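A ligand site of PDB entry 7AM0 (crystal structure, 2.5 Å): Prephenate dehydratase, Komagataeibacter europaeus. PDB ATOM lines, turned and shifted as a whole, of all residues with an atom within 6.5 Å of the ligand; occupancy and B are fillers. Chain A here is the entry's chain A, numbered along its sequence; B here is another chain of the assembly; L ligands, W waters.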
ATOM      1  N   VAL A 201       5.624  -1.715  27.683  1.00  0.00           N
ATOM      2  CA  VAL A 201       5.085  -2.950  27.090  1.00  0.00           C
ATOM      3  C   VAL A 201       6.226  -3.802  26.561  1.00  0.00           C
ATOM      4  O   VAL A 201       7.349  -3.316  26.359  1.00  0.00           O
ATOM      5  CB  VAL A 201       4.057  -2.683  25.971  1.00  0.00           C
ATOM      6  CG1 VAL A 201       2.906  -1.815  26.489  1.00  0.00           C
ATOM      7  CG2 VAL A 201       4.714  -2.055  24.747  1.00  0.00           C
ATOM      8  N   ASN A 202       5.940  -5.085  26.344  1.00  0.00           N
ATOM      9  CA  ASN A 202       6.931  -6.076  25.926  1.00  0.00           C
ATOM     10  C   ASN A 202       7.341  -5.909  24.467  1.00  0.00           C
ATOM     11  O   ASN A 202       6.660  -5.229  23.701  1.00  0.00           O
ATOM     12  CB  ASN A 202       6.397  -7.482  26.170  1.00  0.00           C
ATOM     13  CG  ASN A 202       6.147  -7.753  27.633  1.00  0.00           C
ATOM     14  OD1 ASN A 202       5.158  -8.370  28.005  1.00  0.00           O
ATOM     15  ND2 ASN A 202       7.038  -7.268  28.495  1.00  0.00           N
ATOM     16  N   ASN A 203       8.471  -6.529  24.112  1.00  0.00           N
ATOM     17  CA  ASN A 203       9.019  -6.454  22.760  1.00  0.00           C
ATOM     18  C   ASN A 203       8.475  -7.577  21.881  1.00  0.00           C
ATOM     19  O   ASN A 203       9.196  -8.490  21.473  1.00  0.00           O
ATOM     20  CB  ASN A 203      10.550  -6.497  22.790  1.00  0.00           C
ATOM     21  CG  ASN A 203      11.163  -6.270  21.421  1.00  0.00           C
ATOM     22  OD1 ASN A 203      10.804  -5.321  20.720  1.00  0.00           O
ATOM     23  ND2 ASN A 203      12.088  -7.135  21.027  1.00  0.00           N
ATOM     24  N   GLN A 204       7.169  -7.489  21.588  1.00  0.00           N
ATOM     25  CA  GLN A 204       6.495  -8.416  20.706  1.00  0.00           C
ATOM     26  C   GLN A 204       5.624  -7.629  19.729  1.00  0.00           C
ATOM     27  O   GLN A 204       5.103  -6.574  20.095  1.00  0.00           O
ATOM     28  CB  GLN A 204       5.637  -9.426  21.495  1.00  0.00           C
ATOM     29  CG  GLN A 204       6.387 -10.237  22.541  1.00  0.00           C
ATOM     30  CD  GLN A 204       7.213 -11.356  21.925  1.00  0.00           C
ATOM     31  OE1 GLN A 204       6.658 -12.332  21.421  1.00  0.00           O
ATOM     32  NE2 GLN A 204       8.538 -11.234  21.998  1.00  0.00           N
ATOM     33  N   PRO A 205       5.439  -8.114  18.484  1.00  0.00           N
ATOM     34  CA  PRO A 205       4.522  -7.484  17.535  1.00  0.00           C
ATOM     35  C   PRO A 205       3.150  -7.243  18.173  1.00  0.00           C
ATOM     36  O   PRO A 205       2.590  -8.152  18.785  1.00  0.00           O
ATOM     37  CB  PRO A 205       4.428  -8.505  16.401  1.00  0.00           C
ATOM     38  CG  PRO A 205       5.681  -9.311  16.483  1.00  0.00           C
ATOM     39  CD  PRO A 205       6.107  -9.309  17.927  1.00  0.00           C
ATOM     40  N   GLY A 206       2.634  -6.016  18.043  1.00  0.00           N
ATOM     41  CA  GLY A 206       1.312  -5.663  18.505  1.00  0.00           C
ATOM     42  C   GLY A 206       1.185  -5.233  19.960  1.00  0.00           C
ATOM     43  O   GLY A 206       0.102  -4.861  20.392  1.00  0.00           O
ATOM     44  N   ALA A 207       2.304  -5.296  20.708  1.00  0.00           N
ATOM     45  CA  ALA A 207       2.294  -5.020  22.141  1.00  0.00           C
ATOM     46  C   ALA A 207       1.788  -3.607  22.417  1.00  0.00           C
ATOM     47  O   ALA A 207       0.887  -3.414  23.242  1.00  0.00           O
ATOM     48  CB  ALA A 207       3.682  -5.221  22.725  1.00  0.00           C
ATOM     49  N   LEU A 208       2.365  -2.637  21.693  1.00  0.00           N
ATOM     50  CA  LEU A 208       1.952  -1.239  21.772  1.00  0.00           C
ATOM     51  C   LEU A 208       0.533  -1.074  21.236  1.00  0.00           C
ATOM     52  O   LEU A 208      -0.298  -0.420  21.848  1.00  0.00           O
ATOM     53  CB  LEU A 208       2.936  -0.333  21.018  1.00  0.00           C
ATOM     54  CG  LEU A 208       2.499   1.116  20.730  1.00  0.00           C
ATOM     55  CD1 LEU A 208       2.329   1.915  22.012  1.00  0.00           C
ATOM     56  CD2 LEU A 208       3.431   1.804  19.752  1.00  0.00           C
ATOM     57  N   TYR A 209       0.288  -1.677  20.057  1.00  0.00           N
ATOM     58  CA  TYR A 209      -1.005  -1.644  19.376  1.00  0.00           C
ATOM     59  C   TYR A 209      -2.168  -2.006  20.294  1.00  0.00           C
ATOM     60  O   TYR A 209      -3.175  -1.290  20.327  1.00  0.00           O
ATOM     61  CB  TYR A 209      -0.960  -2.585  18.172  1.00  0.00           C
ATOM     62  CG  TYR A 209      -2.265  -2.847  17.474  1.00  0.00           C
ATOM     63  CD1 TYR A 209      -3.099  -3.876  17.878  1.00  0.00           C
ATOM     64  CD2 TYR A 209      -2.648  -2.064  16.388  1.00  0.00           C
ATOM     65  CE1 TYR A 209      -4.291  -4.139  17.202  1.00  0.00           C
ATOM     66  CE2 TYR A 209      -3.836  -2.313  15.720  1.00  0.00           C
ATOM     67  CZ  TYR A 209      -4.655  -3.352  16.123  1.00  0.00           C
ATOM     68  OH  TYR A 209      -5.827  -3.578  15.454  1.00  0.00           O
ATOM     69  N   LYS A 210      -2.021  -3.106  21.045  1.00  0.00           N
ATOM     70  CA  LYS A 210      -3.019  -3.548  22.020  1.00  0.00           C
ATOM     71  C   LYS A 210      -3.278  -2.480  23.088  1.00  0.00           C
ATOM     72  O   LYS A 210      -4.421  -2.142  23.360  1.00  0.00           O
ATOM     73  CB  LYS A 210      -2.566  -4.824  22.735  1.00  0.00           C
ATOM     74  CG  LYS A 210      -2.704  -6.100  21.945  1.00  0.00           C
ATOM     75  CD  LYS A 210      -2.228  -7.273  22.785  1.00  0.00           C
ATOM     76  CE  LYS A 210      -2.369  -8.597  22.061  1.00  0.00           C
ATOM     77  NZ  LYS A 210      -3.769  -8.840  21.617  1.00  0.00           N
ATOM     78  N   SER A 227       9.074   6.444  22.258  1.00  0.00           N
ATOM     79  CA  SER A 227       9.666   5.227  22.805  1.00  0.00           C
ATOM     80  C   SER A 227      11.094   5.463  23.325  1.00  0.00           C
ATOM     81  O   SER A 227      11.788   6.371  22.853  1.00  0.00           O
ATOM     82  CB  SER A 227       9.711   4.136  21.734  1.00  0.00           C
ATOM     83  OG  SER A 227      10.507   4.533  20.627  1.00  0.00           O
ATOM     84  N   TYR A 228      11.491   4.630  24.297  1.00  0.00           N
ATOM     85  CA  TYR A 228      12.816   4.629  24.873  1.00  0.00           C
ATOM     86  C   TYR A 228      13.318   3.216  25.084  1.00  0.00           C
ATOM     87  O   TYR A 228      12.545   2.325  25.438  1.00  0.00           O
ATOM     88  CB  TYR A 228      12.807   5.352  26.220  1.00  0.00           C
ATOM     89  CG  TYR A 228      12.369   6.795  26.137  1.00  0.00           C
ATOM     90  CD1 TYR A 228      13.266   7.799  25.787  1.00  0.00           C
ATOM     91  CD2 TYR A 228      11.044   7.148  26.383  1.00  0.00           C
ATOM     92  CE1 TYR A 228      12.857   9.125  25.683  1.00  0.00           C
ATOM     93  CE2 TYR A 228      10.628   8.463  26.303  1.00  0.00           C
ATOM     94  CZ  TYR A 228      11.535   9.442  25.945  1.00  0.00           C
ATOM     95  OH  TYR A 228      11.111  10.745  25.866  1.00  0.00           O
ATOM     96  N   ALA A 236      11.594  -5.374  26.668  1.00  0.00           N
ATOM     97  CA  ALA A 236      10.472  -4.454  26.737  1.00  0.00           C
ATOM     98  C   ALA A 236      10.891  -3.074  26.243  1.00  0.00           C
ATOM     99  O   ALA A 236      12.072  -2.831  25.979  1.00  0.00           O
ATOM    100  CB  ALA A 236       9.955  -4.390  28.168  1.00  0.00           C
ATOM    101  N   THR A 237       9.912  -2.169  26.129  1.00  0.00           N
ATOM    102  CA  THR A 237      10.137  -0.797  25.682  1.00  0.00           C
ATOM    103  C   THR A 237       9.236   0.157  26.459  1.00  0.00           C
ATOM    104  O   THR A 237       8.037  -0.104  26.614  1.00  0.00           O
ATOM    105  CB  THR A 237       9.863  -0.650  24.171  1.00  0.00           C
ATOM    106  OG1 THR A 237      10.775  -1.471  23.441  1.00  0.00           O
ATOM    107  CG2 THR A 237      10.016   0.781  23.724  1.00  0.00           C
ATOM    108  N   GLN A 238       9.823   1.248  26.944  1.00  0.00           N
ATOM    109  CA  GLN A 238       9.125   2.258  27.705  1.00  0.00           C
ATOM    110  C   GLN A 238       8.618   3.334  26.758  1.00  0.00           C
ATOM    111  O   GLN A 238       9.247   3.610  25.735  1.00  0.00           O
ATOM    112  CB  GLN A 238      10.045   2.862  28.748  1.00  0.00           C
ATOM    113  CG  GLN A 238       9.325   3.617  29.852  1.00  0.00           C
ATOM    114  CD  GLN A 238      10.302   4.340  30.781  1.00  0.00           C
ATOM    115  OE1 GLN A 238      11.517   4.327  30.579  1.00  0.00           O
ATOM    116  NE2 GLN A 238       9.764   4.989  31.806  1.00  0.00           N
ATOM    117  N   PHE A 239       7.489   3.945  27.117  1.00  0.00           N
ATOM    118  CA  PHE A 239       6.862   5.011  26.340  1.00  0.00           C
ATOM    119  C   PHE A 239       6.509   6.179  27.211  1.00  0.00           C
ATOM    120  O   PHE A 239       6.036   6.006  28.331  1.00  0.00           O
ATOM    121  CB  PHE A 239       5.588   4.511  25.671  1.00  0.00           C
ATOM    122  CG  PHE A 239       5.831   3.638  24.480  1.00  0.00           C
ATOM    123  CD1 PHE A 239       5.980   4.183  23.224  1.00  0.00           C
ATOM    124  CD2 PHE A 239       5.935   2.270  24.626  1.00  0.00           C
ATOM    125  CE1 PHE A 239       6.210   3.385  22.127  1.00  0.00           C
ATOM    126  CE2 PHE A 239       6.166   1.463  23.534  1.00  0.00           C
ATOM    127  CZ  PHE A 239       6.310   2.020  22.281  1.00  0.00           C
ATOM    128  N   LEU B 212      -0.820   1.062  12.446  1.00  0.00           N
ATOM    129  CA  LEU B 212      -0.011   0.006  13.037  1.00  0.00           C
ATOM    130  C   LEU B 212      -0.608  -1.400  12.879  1.00  0.00           C
ATOM    131  O   LEU B 212       0.113  -2.385  12.967  1.00  0.00           O
ATOM    132  CB  LEU B 212       0.210   0.286  14.527  1.00  0.00           C
ATOM    133  CG  LEU B 212       0.977   1.556  14.910  1.00  0.00           C
ATOM    134  CD1 LEU B 212       1.181   1.590  16.419  1.00  0.00           C
ATOM    135  CD2 LEU B 212       2.308   1.662  14.193  1.00  0.00           C
ATOM    136  N   LEU B 215       1.112  -3.944  10.817  1.00  0.00           N
ATOM    137  CA  LEU B 215       2.370  -4.409  11.406  1.00  0.00           C
ATOM    138  C   LEU B 215       2.111  -5.557  12.376  1.00  0.00           C
ATOM    139  O   LEU B 215       2.806  -6.563  12.351  1.00  0.00           O
ATOM    140  CB  LEU B 215       3.100  -3.252  12.103  1.00  0.00           C
ATOM    141  CG  LEU B 215       3.601  -2.098  11.218  1.00  0.00           C
ATOM    142  CD1 LEU B 215       4.128  -0.914  12.015  1.00  0.00           C
ATOM    143  CD2 LEU B 215       4.678  -2.604  10.276  1.00  0.00           C
ATOM    144  N   VAL B 220       5.290  -8.162  12.474  1.00  0.00           N
ATOM    145  CA  VAL B 220       6.435  -7.281  12.337  1.00  0.00           C
ATOM    146  C   VAL B 220       6.649  -6.459  13.613  1.00  0.00           C
ATOM    147  O   VAL B 220       5.733  -5.744  14.062  1.00  0.00           O
ATOM    148  CB  VAL B 220       6.295  -6.357  11.101  1.00  0.00           C
ATOM    149  CG1 VAL B 220       7.335  -5.255  11.107  1.00  0.00           C
ATOM    150  CG2 VAL B 220       6.381  -7.165   9.816  1.00  0.00           C
ATOM    151  N   ASN B 221       7.846  -6.560  14.190  1.00  0.00           N
ATOM    152  CA  ASN B 221       8.181  -5.937  15.466  1.00  0.00           C
ATOM    153  C   ASN B 221       8.811  -4.553  15.303  1.00  0.00           C
ATOM    154  O   ASN B 221       9.807  -4.400  14.589  1.00  0.00           O
ATOM    155  CB  ASN B 221       9.138  -6.848  16.227  1.00  0.00           C
ATOM    156  CG  ASN B 221       9.253  -6.476  17.697  1.00  0.00           C
ATOM    157  OD1 ASN B 221       8.264  -6.511  18.427  1.00  0.00           O
ATOM    158  ND2 ASN B 221      10.475  -6.124  18.125  1.00  0.00           N
ATOM    159  N   MET B 222       8.210  -3.548  15.961  1.00  0.00           N
ATOM    160  CA  MET B 222       8.737  -2.184  16.017  1.00  0.00           C
ATOM    161  C   MET B 222       9.749  -2.075  17.142  1.00  0.00           C
ATOM    162  O   MET B 222       9.530  -2.577  18.238  1.00  0.00           O
ATOM    163  CB  MET B 222       7.616  -1.176  16.278  1.00  0.00           C
ATOM    164  CG  MET B 222       6.858  -0.752  15.040  1.00  0.00           C
ATOM    165  SD  MET B 222       5.298   0.051  15.401  1.00  0.00           S
ATOM    166  CE  MET B 222       5.833   1.511  16.269  1.00  0.00           C
ATOM    167  N   THR B 223      10.863  -1.377  16.873  1.00  0.00           N
ATOM    168  CA  THR B 223      11.928  -1.173  17.855  1.00  0.00           C
ATOM    169  C   THR B 223      11.960   0.261  18.383  1.00  0.00           C
ATOM    170  O   THR B 223      12.381   0.486  19.519  1.00  0.00           O
ATOM    171  CB  THR B 223      13.292  -1.570  17.288  1.00  0.00           C
ATOM    172  OG1 THR B 223      13.434  -1.032  15.971  1.00  0.00           O
ATOM    173  CG2 THR B 223      13.402  -3.074  17.207  1.00  0.00           C
ATOM    174  N   ARG B 224      11.474   1.217  17.579  1.00  0.00           N
ATOM    175  CA  ARG B 224      11.364   2.608  17.993  1.00  0.00           C
ATOM    176  C   ARG B 224      10.181   3.303  17.336  1.00  0.00           C
ATOM    177  O   ARG B 224       9.811   2.989  16.215  1.00  0.00           O
ATOM    178  CB  ARG B 224      12.635   3.373  17.646  1.00  0.00           C
ATOM    179  CG  ARG B 224      12.750   4.713  18.338  1.00  0.00           C
ATOM    180  CD  ARG B 224      13.815   5.575  17.690  1.00  0.00           C
ATOM    181  NE  ARG B 224      13.863   6.907  18.305  1.00  0.00           N
ATOM    182  CZ  ARG B 224      14.654   7.878  17.880  1.00  0.00           C
ATOM    183  NH1 ARG B 224      15.461   7.698  16.835  1.00  0.00           N
ATOM    184  NH2 ARG B 224      14.635   9.066  18.483  1.00  0.00           N
ATOM    185  N   LEU B 225       9.604   4.276  18.066  1.00  0.00           N
ATOM    186  CA  LEU B 225       8.544   5.143  17.569  1.00  0.00           C
ATOM    187  C   LEU B 225       8.595   6.479  18.314  1.00  0.00           C
ATOM    188  O   LEU B 225       8.743   6.503  19.549  1.00  0.00           O
ATOM    189  CB  LEU B 225       7.182   4.470  17.773  1.00  0.00           C
ATOM    190  CG  LEU B 225       5.973   5.185  17.167  1.00  0.00           C
ATOM    191  CD1 LEU B 225       6.096   5.232  15.647  1.00  0.00           C
ATOM    192  CD2 LEU B 225       4.676   4.529  17.588  1.00  0.00           C
ATOM    193  N   ASP B 242      11.313   3.018  13.719  1.00  0.00           N
ATOM    194  CA  ASP B 242      12.244   1.935  13.429  1.00  0.00           C
ATOM    195  C   ASP B 242      11.438   0.637  13.502  1.00  0.00           C
ATOM    196  O   ASP B 242      10.741   0.389  14.479  1.00  0.00           O
ATOM    197  CB  ASP B 242      13.371   1.854  14.451  1.00  0.00           C
ATOM    198  CG  ASP B 242      14.375   2.993  14.351  1.00  0.00           C
ATOM    199  OD1 ASP B 242      14.276   3.843  13.429  1.00  0.00           O
ATOM    200  OD2 ASP B 242      15.287   3.039  15.212  1.00  0.00           O
HETATM  201  N1  LIG L   1       7.721  -4.002  19.836  1.00  0.00           N
HETATM  202  C1  LIG L   1       6.347  -3.765  20.343  1.00  0.00           C
HETATM  203  C2  LIG L   1       5.284  -3.582  19.145  1.00  0.00           C
HETATM  204  O1  LIG L   1       5.613  -3.829  17.980  1.00  0.00           O
HETATM  205  C3  LIG L   1       6.340  -2.511  21.235  1.00  0.00           C
HETATM  206  C4  LIG L   1       7.134  -1.376  20.661  1.00  0.00           C
HETATM  207  C5  LIG L   1       6.575  -0.513  19.739  1.00  0.00           C
HETATM  208  C6  LIG L   1       8.457  -1.176  21.048  1.00  0.00           C
HETATM  209  C7  LIG L   1       7.306   0.540  19.215  1.00  0.00           C
HETATM  210  C8  LIG L   1       9.202  -0.134  20.523  1.00  0.00           C
HETATM  211  C9  LIG L   1       8.622   0.719  19.606  1.00  0.00           C
HETATM  212  O2  LIG L   1       4.115  -3.195  19.337  1.00  0.00           O
HETATM  213  O   HOH W   1       3.862  -3.941  16.005  1.00  0.00           O
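N of Met 222 of chain B lies within hydrogen-bond range of O1 of the ligand (3.3 Å).
The side-chain amide oxygen (OD1) of Asn 203 sits at hydrogen-bond distance from a nitrogen (N1) of the ligand (3.5 Å).
A nitrogen (N1) of the ligand lies within hydrogen-bond range of the backbone carbonyl oxygen (O) of Met 222 of chain B (2.8 Å).
The backbone NH (N) of Gly 206 lies within hydrogen-bond range of an oxygen (O2) of the ligand (3.4 Å).
O2 of the ligand is in hydrogen-bond range of N of Leu 208 (3.0 Å).
An oxygen (O2) of the ligand lies within hydrogen-bond range of the backbone NH (N) of Ala 207.
OD1 of Asn 221 of chain B sits at hydrogen-bond distance from N1 of the ligand, 2.9 Å away.
The backbone NH (N) of Asp 242 of chain B is in hydrogen-bond range of the backbone carbonyl oxygen (O) of Arg 224 of chain B (2.9 Å).
OD1 of Asn 221 of chain B sits close to N of Gln 204 (3.5 Å).
The side-chain amide nitrogen (ND2) of Asn 221 of chain B lies within hydrogen-bond range of the side-chain amide oxygen (OD1) of Asn 203, at 2.7 Å.
N of Thr 237 is in hydrogen-bond range of O of Val 201 (2.8 Å).
The backbone NH (N) of Leu 225 of chain B is in hydrogen-bond range of the side-chain hydroxyl (OG) of Ser 227 (2.7 Å).
N of Thr 223 of chain B lies within hydrogen-bond range of O of Asp 242 of chain B, 3.0 Å away.
Merely in contact with the ligand: Val 201 (3.9 Å), Asn 202 (3.7 Å), Gln 204 (3.1 Å), Pro 205 (3.8 Å), Thr 237 (3.3 Å), Phe 239 (3.5 Å), Thr 223 of chain B (3.4 Å), Arg 224 of chain B (3.5 Å) and Leu 225 of chain B (3.999 Å).
Hydrophobic or aromatic side chains within 4 Å of the ligand: Val 201, Ala 207, Leu 208, Phe 239 and Met 222 of chain B.
Within 4 Å of the ligand: Val 201, Asn 202, Asn 203, Gln 204, Pro 205, Gly 206, Ala 207, Leu 208, Thr 237, Phe 239, Asn 221 of chain B, Met 222 of chain B, Thr 223 of chain B, Arg 224 of chain B and Leu 225 of chain B.
The nearest printed residue that does not touch the ligand is Ser 227 (4.2 Å).
Water W1 lies within hydrogen-bond range of O1 of the ligand, N of Gly 206 and O of Val 220 of chain B.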
